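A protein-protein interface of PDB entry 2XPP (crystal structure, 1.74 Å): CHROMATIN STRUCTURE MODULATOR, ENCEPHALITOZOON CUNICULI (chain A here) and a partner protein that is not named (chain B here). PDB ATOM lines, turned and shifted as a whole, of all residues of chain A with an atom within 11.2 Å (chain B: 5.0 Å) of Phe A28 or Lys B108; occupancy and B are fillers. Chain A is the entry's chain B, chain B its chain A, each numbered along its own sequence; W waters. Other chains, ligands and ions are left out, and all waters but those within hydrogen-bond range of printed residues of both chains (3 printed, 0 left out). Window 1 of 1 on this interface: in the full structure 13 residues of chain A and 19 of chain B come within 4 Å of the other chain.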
ATOM      1  N   ASP A  19     -21.670 -14.396 -19.059  1.00  0.00           N
ATOM      2  CA  ASP A  19     -22.506 -13.269 -19.443  1.00  0.00           C
ATOM      3  C   ASP A  19     -23.841 -13.241 -18.706  1.00  0.00           C
ATOM      4  O   ASP A  19     -24.308 -12.179 -18.340  1.00  0.00           O
ATOM      5  CB  ASP A  19     -22.693 -13.261 -20.937  1.00  0.00           C
ATOM      6  CG  ASP A  19     -21.359 -13.041 -21.674  1.00  0.00           C
ATOM      7  OD1 ASP A  19     -20.470 -12.335 -21.114  1.00  0.00           O
ATOM      8  OD2 ASP A  19     -21.201 -13.546 -22.806  1.00  0.00           O
ATOM      9  N   ARG A  20     -24.428 -14.413 -18.476  1.00  0.00           N
ATOM     10  CA  ARG A  20     -25.615 -14.467 -17.631  1.00  0.00           C
ATOM     11  C   ARG A  20     -25.295 -13.924 -16.228  1.00  0.00           C
ATOM     12  O   ARG A  20     -26.110 -13.214 -15.654  1.00  0.00           O
ATOM     13  CB  ARG A  20     -26.134 -15.902 -17.511  1.00  0.00           C
ATOM     14  CG  ARG A  20     -26.731 -16.455 -18.797  1.00  0.00           C
ATOM     15  CD  ARG A  20     -27.591 -15.402 -19.478  1.00  0.00           C
ATOM     16  NE  ARG A  20     -28.546 -15.991 -20.414  1.00  0.00           N
ATOM     17  CZ  ARG A  20     -28.310 -16.220 -21.702  1.00  0.00           C
ATOM     18  NH1 ARG A  20     -27.135 -15.903 -22.242  1.00  0.00           N
ATOM     19  NH2 ARG A  20     -29.254 -16.777 -22.454  1.00  0.00           N
ATOM     20  N   ASP A  21     -24.124 -14.285 -15.671  1.00  0.00           N
ATOM     21  CA  ASP A  21     -23.753 -13.797 -14.322  1.00  0.00           C
ATOM     22  C   ASP A  21     -23.633 -12.289 -14.323  1.00  0.00           C
ATOM     23  O   ASP A  21     -24.031 -11.629 -13.353  1.00  0.00           O
ATOM     24  CB  ASP A  21     -22.437 -14.410 -13.824  1.00  0.00           C
ATOM     25  CG  ASP A  21     -22.601 -15.849 -13.364  1.00  0.00           C
ATOM     26  OD1 ASP A  21     -23.721 -16.387 -13.469  1.00  0.00           O
ATOM     27  OD2 ASP A  21     -21.631 -16.431 -12.857  1.00  0.00           O
ATOM     28  N   SER A  22     -23.082 -11.744 -15.406  1.00  0.00           N
ATOM     29  CA  SER A  22     -22.878 -10.297 -15.464  1.00  0.00           C
ATOM     30  C   SER A  22     -24.257  -9.606 -15.454  1.00  0.00           C
ATOM     31  O   SER A  22     -24.417  -8.563 -14.824  1.00  0.00           O
ATOM     32  CB  SER A  22     -22.033  -9.915 -16.653  1.00  0.00           C
ATOM     33  OG  SER A  22     -20.691 -10.367 -16.444  1.00  0.00           O
ATOM     34  N   LEU A  23     -25.250 -10.224 -16.101  1.00  0.00           N
ATOM     35  CA  LEU A  23     -26.611  -9.636 -16.094  1.00  0.00           C
ATOM     36  C   LEU A  23     -27.238  -9.803 -14.717  1.00  0.00           C
ATOM     37  O   LEU A  23     -27.922  -8.878 -14.208  1.00  0.00           O
ATOM     38  CB  LEU A  23     -27.496 -10.205 -17.225  1.00  0.00           C
ATOM     39  CG  LEU A  23     -28.990  -9.847 -17.151  1.00  0.00           C
ATOM     40  CD1 LEU A  23     -29.261  -8.308 -17.215  1.00  0.00           C
ATOM     41  CD2 LEU A  23     -29.738 -10.528 -18.252  1.00  0.00           C
ATOM     42  N   PHE A  24     -26.995 -10.965 -14.107  1.00  0.00           N
ATOM     43  CA  PHE A  24     -27.406 -11.237 -12.714  1.00  0.00           C
ATOM     44  C   PHE A  24     -26.838 -10.154 -11.771  1.00  0.00           C
ATOM     45  O   PHE A  24     -27.583  -9.603 -10.920  1.00  0.00           O
ATOM     46  CB  PHE A  24     -26.949 -12.633 -12.312  1.00  0.00           C
ATOM     47  CG  PHE A  24     -27.426 -13.072 -10.970  1.00  0.00           C
ATOM     48  CD1 PHE A  24     -28.650 -13.731 -10.844  1.00  0.00           C
ATOM     49  CD2 PHE A  24     -26.628 -12.896  -9.830  1.00  0.00           C
ATOM     50  CE1 PHE A  24     -29.095 -14.176  -9.608  1.00  0.00           C
ATOM     51  CE2 PHE A  24     -27.054 -13.353  -8.585  1.00  0.00           C
ATOM     52  CZ  PHE A  24     -28.306 -13.985  -8.469  1.00  0.00           C
ATOM     53  N   PHE A  25     -25.556  -9.835 -11.941  1.00  0.00           N
ATOM     54  CA  PHE A  25     -24.992  -8.721 -11.128  1.00  0.00           C
ATOM     55  C   PHE A  25     -25.616  -7.358 -11.451  1.00  0.00           C
ATOM     56  O   PHE A  25     -25.778  -6.522 -10.534  1.00  0.00           O
ATOM     57  CB  PHE A  25     -23.469  -8.676 -11.136  1.00  0.00           C
ATOM     58  CG  PHE A  25     -22.811  -9.967 -10.706  1.00  0.00           C
ATOM     59  CD1 PHE A  25     -23.262 -10.673  -9.571  1.00  0.00           C
ATOM     60  CD2 PHE A  25     -21.710 -10.469 -11.430  1.00  0.00           C
ATOM     61  CE1 PHE A  25     -22.638 -11.891  -9.182  1.00  0.00           C
ATOM     62  CE2 PHE A  25     -21.076 -11.679 -11.053  1.00  0.00           C
ATOM     63  CZ  PHE A  25     -21.547 -12.389  -9.921  1.00  0.00           C
ATOM     64  N   GLU A  26     -26.008  -7.108 -12.692  1.00  0.00           N
ATOM     65  CA  GLU A  26     -26.607  -5.795 -13.004  1.00  0.00           C
ATOM     66  C   GLU A  26     -27.907  -5.622 -12.220  1.00  0.00           C
ATOM     67  O   GLU A  26     -28.247  -4.514 -11.759  1.00  0.00           O
ATOM     68  CB  GLU A  26     -26.934  -5.647 -14.482  1.00  0.00           C
ATOM     69  CG  GLU A  26     -25.802  -5.347 -15.389  1.00  0.00           C
ATOM     70  CD  GLU A  26     -26.290  -4.951 -16.766  1.00  0.00           C
ATOM     71  OE1 GLU A  26     -26.641  -3.758 -16.942  1.00  0.00           O
ATOM     72  OE2 GLU A  26     -26.293  -5.831 -17.675  1.00  0.00           O
ATOM     73  N   ILE A  27     -28.620  -6.731 -12.108  1.00  0.00           N
ATOM     74  CA  ILE A  27     -29.897  -6.798 -11.390  1.00  0.00           C
ATOM     75  C   ILE A  27     -29.798  -6.816  -9.865  1.00  0.00           C
ATOM     76  O   ILE A  27     -30.497  -6.042  -9.191  1.00  0.00           O
ATOM     77  CB  ILE A  27     -30.754  -8.004 -11.921  1.00  0.00           C
ATOM     78  CG1 ILE A  27     -31.126  -7.721 -13.381  1.00  0.00           C
ATOM     79  CG2 ILE A  27     -32.059  -8.276 -11.078  1.00  0.00           C
ATOM     80  CD1 ILE A  27     -31.626  -8.969 -14.083  1.00  0.00           C
ATOM     81  N   PHE A  28     -28.996  -7.726  -9.330  1.00  0.00           N
ATOM     82  CA  PHE A  28     -29.045  -8.052  -7.897  1.00  0.00           C
ATOM     83  C   PHE A  28     -27.867  -7.492  -7.127  1.00  0.00           C
ATOM     84  O   PHE A  28     -27.896  -7.494  -5.873  1.00  0.00           O
ATOM     85  CB  PHE A  28     -29.094  -9.565  -7.683  1.00  0.00           C
ATOM     86  CG  PHE A  28     -30.353 -10.195  -8.165  1.00  0.00           C
ATOM     87  CD1 PHE A  28     -30.351 -11.038  -9.273  1.00  0.00           C
ATOM     88  CD2 PHE A  28     -31.569  -9.923  -7.527  1.00  0.00           C
ATOM     89  CE1 PHE A  28     -31.565 -11.630  -9.695  1.00  0.00           C
ATOM     90  CE2 PHE A  28     -32.730 -10.476  -7.947  1.00  0.00           C
ATOM     91  CZ  PHE A  28     -32.735 -11.340  -9.049  1.00  0.00           C
ATOM     92  N   GLY A  29     -26.877  -7.039  -7.888  1.00  0.00           N
ATOM     93  CA  GLY A  29     -25.580  -6.579  -7.416  1.00  0.00           C
ATOM     94  C   GLY A  29     -24.931  -7.776  -6.769  1.00  0.00           C
ATOM     95  O   GLY A  29     -25.276  -8.928  -7.085  1.00  0.00           O
ATOM     96  N   THR A  30     -24.057  -7.513  -5.803  1.00  0.00           N
ATOM     97  CA  THR A  30     -23.287  -8.583  -5.187  1.00  0.00           C
ATOM     98  C   THR A  30     -23.553  -8.843  -3.716  1.00  0.00           C
ATOM     99  O   THR A  30     -22.713  -9.456  -3.058  1.00  0.00           O
ATOM    100  CB  THR A  30     -21.784  -8.313  -5.370  1.00  0.00           C
ATOM    101  OG1 THR A  30     -21.474  -7.000  -4.863  1.00  0.00           O
ATOM    102  CG2 THR A  30     -21.433  -8.408  -6.863  1.00  0.00           C
ATOM    103  N   GLY A  31     -24.692  -8.379  -3.194  1.00  0.00           N
ATOM    104  CA  GLY A  31     -25.018  -8.543  -1.769  1.00  0.00           C
ATOM    105  C   GLY A  31     -24.310  -7.580  -0.831  1.00  0.00           C
ATOM    106  O   GLY A  31     -24.360  -7.727   0.396  1.00  0.00           O
ATOM    107  N   GLU A  32     -23.639  -6.583  -1.389  1.00  0.00           N
ATOM    108  CA  GLU A  32     -22.851  -5.668  -0.575  1.00  0.00           C
ATOM    109  C   GLU A  32     -23.629  -4.429  -0.238  1.00  0.00           C
ATOM    110  O   GLU A  32     -23.371  -3.781   0.763  1.00  0.00           O
ATOM    111  CB  GLU A  32     -21.562  -5.260  -1.303  1.00  0.00           C
ATOM    112  CG  GLU A  32     -20.588  -6.400  -1.617  1.00  0.00           C
ATOM    113  CD  GLU A  32     -19.918  -7.017  -0.379  1.00  0.00           C
ATOM    114  OE1 GLU A  32     -19.720  -6.310   0.646  1.00  0.00           O
ATOM    115  OE2 GLU A  32     -19.593  -8.220  -0.450  1.00  0.00           O
ATOM    116  N   GLU A  33     -24.590  -4.123  -1.096  1.00  0.00           N
ATOM    117  CA  GLU A  33     -25.299  -2.853  -1.134  1.00  0.00           C
ATOM    118  C   GLU A  33     -25.778  -2.379   0.252  1.00  0.00           C
ATOM    119  O   GLU A  33     -25.573  -1.220   0.620  1.00  0.00           O
ATOM    120  CB  GLU A  33     -26.458  -2.954  -2.147  1.00  0.00           C
ATOM    121  CG  GLU A  33     -26.019  -3.090  -3.649  1.00  0.00           C
ATOM    122  CD  GLU A  33     -25.427  -4.467  -4.040  1.00  0.00           C
ATOM    123  OE1 GLU A  33     -26.133  -5.512  -3.851  1.00  0.00           O
ATOM    124  OE2 GLU A  33     -24.255  -4.510  -4.545  1.00  0.00           O
ATOM    125  N   TYR A  34     -26.391  -3.292   1.013  1.00  0.00           N
ATOM    126  CA  TYR A  34     -26.947  -2.979   2.331  1.00  0.00           C
ATOM    127  C   TYR A  34     -26.257  -3.671   3.517  1.00  0.00           C
ATOM    128  O   TYR A  34     -26.747  -3.627   4.643  1.00  0.00           O
ATOM    129  CB  TYR A  34     -28.466  -3.269   2.327  1.00  0.00           C
ATOM    130  CG  TYR A  34     -29.181  -2.578   1.172  1.00  0.00           C
ATOM    131  CD1 TYR A  34     -29.522  -1.204   1.231  1.00  0.00           C
ATOM    132  CD2 TYR A  34     -29.476  -3.278  -0.004  1.00  0.00           C
ATOM    133  CE1 TYR A  34     -30.162  -0.562   0.158  1.00  0.00           C
ATOM    134  CE2 TYR A  34     -30.102  -2.642  -1.067  1.00  0.00           C
ATOM    135  CZ  TYR A  34     -30.458  -1.311  -0.983  1.00  0.00           C
ATOM    136  OH  TYR A  34     -31.071  -0.695  -2.033  1.00  0.00           O
ATOM    137  N   ARG A  35     -25.076  -4.228   3.296  1.00  0.00           N
ATOM    138  CA  ARG A  35     -24.382  -4.931   4.373  1.00  0.00           C
ATOM    139  C   ARG A  35     -24.155  -4.003   5.558  1.00  0.00           C
ATOM    140  O   ARG A  35     -24.091  -4.459   6.713  1.00  0.00           O
ATOM    141  CB  ARG A  35     -23.043  -5.514   3.899  1.00  0.00           C
ATOM    142  CG  ARG A  35     -22.391  -6.492   4.886  1.00  0.00           C
ATOM    143  CD  ARG A  35     -21.425  -7.456   4.189  1.00  0.00           C
ATOM    144  NE  ARG A  35     -21.989  -7.921   2.913  1.00  0.00           N
ATOM    145  CZ  ARG A  35     -21.445  -8.845   2.117  1.00  0.00           C
ATOM    146  NH1 ARG A  35     -20.306  -9.444   2.456  1.00  0.00           N
ATOM    147  NH2 ARG A  35     -22.051  -9.172   0.977  1.00  0.00           N
ATOM    148  N   TYR A  36     -24.065  -2.702   5.266  1.00  0.00           N
ATOM    149  CA  TYR A  36     -23.724  -1.710   6.284  1.00  0.00           C
ATOM    150  C   TYR A  36     -24.735  -1.766   7.430  1.00  0.00           C
ATOM    151  O   TYR A  36     -24.430  -1.362   8.537  1.00  0.00           O
ATOM    152  CB  TYR A  36     -23.600  -0.293   5.684  1.00  0.00           C
ATOM    153  CG  TYR A  36     -24.904   0.325   5.289  1.00  0.00           C
ATOM    154  CD1 TYR A  36     -25.654   1.048   6.224  1.00  0.00           C
ATOM    155  CD2 TYR A  36     -25.413   0.179   3.997  1.00  0.00           C
ATOM    156  CE1 TYR A  36     -26.830   1.607   5.900  1.00  0.00           C
ATOM    157  CE2 TYR A  36     -26.628   0.726   3.654  1.00  0.00           C
ATOM    158  CZ  TYR A  36     -27.334   1.442   4.612  1.00  0.00           C
ATOM    159  OH  TYR A  36     -28.526   1.990   4.282  1.00  0.00           O
ATOM    160  N   VAL A  37     -25.927  -2.295   7.134  1.00  0.00           N
ATOM    161  CA  VAL A  37     -27.050  -2.419   8.075  1.00  0.00           C
ATOM    162  C   VAL A  37     -26.740  -3.373   9.226  1.00  0.00           C
ATOM    163  O   VAL A  37     -27.182  -3.172  10.365  1.00  0.00           O
ATOM    164  CB  VAL A  37     -28.293  -2.888   7.293  1.00  0.00           C
ATOM    165  CG1 VAL A  37     -29.415  -3.254   8.199  1.00  0.00           C
ATOM    166  CG2 VAL A  37     -28.714  -1.780   6.405  1.00  0.00           C
ATOM    167  N   GLY B 105     -32.996  -1.112  -9.834  1.00  0.00           N
ATOM    168  CA  GLY B 105     -32.193  -1.728  -8.733  1.00  0.00           C
ATOM    169  C   GLY B 105     -32.984  -2.313  -7.584  1.00  0.00           C
ATOM    170  O   GLY B 105     -32.435  -2.641  -6.517  1.00  0.00           O
ATOM    171  N   VAL B 106     -34.287  -2.480  -7.798  1.00  0.00           N
ATOM    172  CA  VAL B 106     -35.137  -3.042  -6.718  1.00  0.00           C
ATOM    173  C   VAL B 106     -34.710  -4.465  -6.348  1.00  0.00           C
ATOM    174  O   VAL B 106     -34.897  -4.880  -5.192  1.00  0.00           O
ATOM    175  CB  VAL B 106     -36.655  -2.919  -7.056  1.00  0.00           C
ATOM    176  CG1 VAL B 106     -37.060  -3.849  -8.194  1.00  0.00           C
ATOM    177  CG2 VAL B 106     -37.522  -3.233  -5.799  1.00  0.00           C
ATOM    178  N   GLY B 107     -34.130  -5.210  -7.311  1.00  0.00           N
ATOM    179  CA  GLY B 107     -33.561  -6.498  -6.991  1.00  0.00           C
ATOM    180  C   GLY B 107     -32.546  -6.469  -5.849  1.00  0.00           C
ATOM    181  O   GLY B 107     -32.434  -7.458  -5.104  1.00  0.00           O
ATOM    182  N   LYS B 108     -31.823  -5.360  -5.716  1.00  0.00           N
ATOM    183  CA  LYS B 108     -30.745  -5.289  -4.730  1.00  0.00           C
ATOM    184  C   LYS B 108     -31.314  -5.276  -3.325  1.00  0.00           C
ATOM    185  O   LYS B 108     -30.771  -5.941  -2.454  1.00  0.00           O
ATOM    186  CB  LYS B 108     -29.832  -4.111  -4.984  1.00  0.00           C
ATOM    187  CG  LYS B 108     -29.102  -4.327  -6.304  1.00  0.00           C
ATOM    188  CD  LYS B 108     -28.470  -3.119  -6.775  1.00  0.00           C
ATOM    189  CE  LYS B 108     -27.709  -3.398  -8.051  1.00  0.00           C
ATOM    190  NZ  LYS B 108     -27.046  -2.161  -8.411  1.00  0.00           N
ATOM    191  N   ILE B 109     -32.388  -4.525  -3.110  1.00  0.00           N
ATOM    192  CA  ILE B 109     -33.006  -4.516  -1.753  1.00  0.00           C
ATOM    193  C   ILE B 109     -33.752  -5.822  -1.479  1.00  0.00           C
ATOM    194  O   ILE B 109     -33.671  -6.356  -0.375  1.00  0.00           O
ATOM    195  CB  ILE B 109     -33.882  -3.259  -1.463  1.00  0.00           C
ATOM    196  CG1 ILE B 109     -34.267  -3.185   0.047  1.00  0.00           C
ATOM    197  CG2 ILE B 109     -35.186  -3.226  -2.325  1.00  0.00           C
ATOM    198  CD1 ILE B 109     -33.086  -3.105   1.054  1.00  0.00           C
ATOM    199  N   VAL B 110     -34.410  -6.373  -2.501  1.00  0.00           N
ATOM    200  CA  VAL B 110     -35.078  -7.666  -2.297  1.00  0.00           C
ATOM    201  C   VAL B 110     -34.049  -8.763  -2.011  1.00  0.00           C
ATOM    202  O   VAL B 110     -34.289  -9.615  -1.141  1.00  0.00           O
ATOM    203  CB  VAL B 110     -35.990  -8.022  -3.486  1.00  0.00           C
ATOM    204  CG1 VAL B 110     -36.570  -9.469  -3.317  1.00  0.00           C
ATOM    205  CG2 VAL B 110     -37.127  -6.933  -3.617  1.00  0.00           C
ATOM    206  N   TYR B 111     -32.903  -8.710  -2.720  1.00  0.00           N
ATOM    207  CA  TYR B 111     -31.832  -9.638  -2.467  1.00  0.00           C
ATOM    208  C   TYR B 111     -31.389  -9.523  -0.999  1.00  0.00           C
ATOM    209  O   TYR B 111     -31.198 -10.550  -0.307  1.00  0.00           O
ATOM    210  CB  TYR B 111     -30.672  -9.483  -3.463  1.00  0.00           C
ATOM    211  CG  TYR B 111     -29.640 -10.553  -3.201  1.00  0.00           C
ATOM    212  CD1 TYR B 111     -29.833 -11.862  -3.667  1.00  0.00           C
ATOM    213  CD2 TYR B 111     -28.539 -10.285  -2.378  1.00  0.00           C
ATOM    214  CE1 TYR B 111     -28.917 -12.866  -3.380  1.00  0.00           C
ATOM    215  CE2 TYR B 111     -27.617 -11.283  -2.075  1.00  0.00           C
ATOM    216  CZ  TYR B 111     -27.809 -12.563  -2.594  1.00  0.00           C
ATOM    217  OH  TYR B 111     -26.880 -13.550  -2.312  1.00  0.00           O
ATOM    218  N   PHE B 112     -31.253  -8.276  -0.509  1.00  0.00           N
ATOM    219  CA  PHE B 112     -30.856  -8.115   0.872  1.00  0.00           C
ATOM    220  C   PHE B 112     -31.877  -8.747   1.839  1.00  0.00           C
ATOM    221  O   PHE B 112     -31.500  -9.411   2.816  1.00  0.00           O
ATOM    222  CB  PHE B 112     -30.620  -6.638   1.216  1.00  0.00           C
ATOM    223  CG  PHE B 112     -30.305  -6.439   2.677  1.00  0.00           C
ATOM    224  CD1 PHE B 112     -29.111  -6.945   3.232  1.00  0.00           C
ATOM    225  CD2 PHE B 112     -31.222  -5.819   3.481  1.00  0.00           C
ATOM    226  CE1 PHE B 112     -28.839  -6.784   4.625  1.00  0.00           C
ATOM    227  CE2 PHE B 112     -30.974  -5.662   4.854  1.00  0.00           C
ATOM    228  CZ  PHE B 112     -29.805  -6.148   5.415  1.00  0.00           C
ATOM    229  N   VAL B 131     -36.693 -13.323  -5.633  1.00  0.00           N
ATOM    230  CA  VAL B 131     -35.371 -13.368  -6.301  1.00  0.00           C
ATOM    231  C   VAL B 131     -35.367 -14.520  -7.290  1.00  0.00           C
ATOM    232  O   VAL B 131     -34.896 -14.393  -8.426  1.00  0.00           O
ATOM    233  CB  VAL B 131     -34.181 -13.527  -5.291  1.00  0.00           C
ATOM    234  CG1 VAL B 131     -32.820 -13.810  -5.988  1.00  0.00           C
ATOM    235  CG2 VAL B 131     -34.045 -12.313  -4.426  1.00  0.00           C
ATOM    236  N   TRP B 134     -37.462 -13.535 -10.426  1.00  0.00           N
ATOM    237  CA  TRP B 134     -36.748 -12.534 -11.257  1.00  0.00           C
ATOM    238  C   TRP B 134     -35.473 -13.080 -11.880  1.00  0.00           C
ATOM    239  O   TRP B 134     -35.038 -12.588 -12.945  1.00  0.00           O
ATOM    240  CB  TRP B 134     -36.427 -11.310 -10.439  1.00  0.00           C
ATOM    241  CG  TRP B 134     -37.666 -10.565 -10.020  1.00  0.00           C
ATOM    242  CD1 TRP B 134     -38.938 -10.743 -10.499  1.00  0.00           C
ATOM    243  CD2 TRP B 134     -37.738  -9.554  -9.028  1.00  0.00           C
ATOM    244  NE1 TRP B 134     -39.811  -9.879  -9.836  1.00  0.00           N
ATOM    245  CE2 TRP B 134     -39.092  -9.151  -8.926  1.00  0.00           C
ATOM    246  CE3 TRP B 134     -36.793  -8.961  -8.186  1.00  0.00           C
ATOM    247  CZ2 TRP B 134     -39.518  -8.138  -8.032  1.00  0.00           C
ATOM    248  CZ3 TRP B 134     -37.227  -7.952  -7.297  1.00  0.00           C
ATOM    249  CH2 TRP B 134     -38.576  -7.562  -7.240  1.00  0.00           C
ATOM    250  N   THR B 135     -34.849 -14.084 -11.238  1.00  0.00           N
ATOM    251  CA  THR B 135     -33.664 -14.742 -11.880  1.00  0.00           C
ATOM    252  C   THR B 135     -33.986 -15.322 -13.246  1.00  0.00           C
ATOM    253  O   THR B 135     -33.110 -15.358 -14.118  1.00  0.00           O
ATOM    254  CB  THR B 135     -32.980 -15.784 -10.951  1.00  0.00           C
ATOM    255  OG1 THR B 135     -32.592 -15.109  -9.748  1.00  0.00           O
ATOM    256  CG2 THR B 135     -31.760 -16.452 -11.640  1.00  0.00           C
HETATM  257  O   HOH W   1     -32.887  -4.903  -9.732  1.00  0.00           O
HETATM  258  O   HOH W   2     -25.316  -3.626 -10.355  1.00  0.00           O
HETATM  259  O   HOH W   3     -28.156  -6.646  -1.867  1.00  0.00           O
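Among the printed residues, pairs that only touch across the chains: Phe A24 with Thr B135, Glu A26 with Lys B108, Ile A27 with Gly B107, Ile A27 with Lys B108, Phe A28 with Gly B107, Phe A28 with Lys B108, Phe A28 with Val B131, Phe A28 with Trp B134, Phe A28 with Thr B135, Gly A29 with Lys B108, Gly A31 with Tyr B111, Glu A33 with Lys B108, Tyr A34 with Lys B108, Tyr A34 with Ile B109 and Tyr A34 with Phe B112.
Hydrophobic or aromatic side chains of chain B within 4 Å of the printed part of chain A: Ile B109, Tyr B111, Phe B112, Val B131 and Trp B134.
Of the 19 printed residues of chain A, 8 touch a printed residue of chain B.
Asp A21 touches none of the printed residues of chain B.
Phe A25 touches none of the printed residues of chain B.
Of the printed residues of chain B, Glu A26 touches Lys B108.
Phe A28 touches just these residues of chain B: Gly B107 (3.6 Å), Lys B108 (3.4 Å), Val B131 (3.8 Å), Trp B134 (3.9 Å) and Thr B135 (3.6 Å).
Of the printed residues of chain B, Tyr A34 touches Lys B108, Ile B109 and Phe B112.
No residue of chain A comes within 4 Å of Val B106.
Lys B108 touches just these residues of chain A: Glu A26, Ile A27, Phe A28, Gly A29, Glu A33 and Tyr A34.
Printed residues of chain A within 4 Å of Ile B109: Tyr A34.
No residue of chain A comes within 4 Å of Val B110.
Of chain A, only Gly A31 comes within 4 Å of Tyr B111.
Val B131 touches just one residue of chain A: Phe A28.
Of the printed residues of chain A, Trp B134 touches Phe A28 (3.9 Å).
Printed residues of chain A within 4 Å of Thr B135: Phe A24 and Phe A28.
The nearest printed residue of chain B that does not touch Gly A31 is Phe B112 (5.6 Å).
O of Val B131 lies within hydrogen-bond range of OG1 of Thr B135, 2.8 Å away.
The backbone carbonyl oxygen of Gly A31 sits at hydrogen-bond distance from the guanidinium group of Arg A35.
N of Gly A31 sits at hydrogen-bond distance from OE1 of Glu A33 (3.3 Å).
The backbone NH of Thr A30 is in hydrogen-bond range of the side-chain carboxylate of Glu A33 (3.3 Å).
Water W1 lies within hydrogen-bond range of O of Ile A27 (2.7 Å), N of Gly B107 (2.7 Å) and N of Val B106 (3.4 Å).
Water W3 bridges O of Lys B108 and OE1 of Glu A33.
Water W2 lies within hydrogen-bond range of O of Phe A25 (2.9 Å), NZ of Lys B108 (3.0 Å) and O of Glu A26 (3.4 Å).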
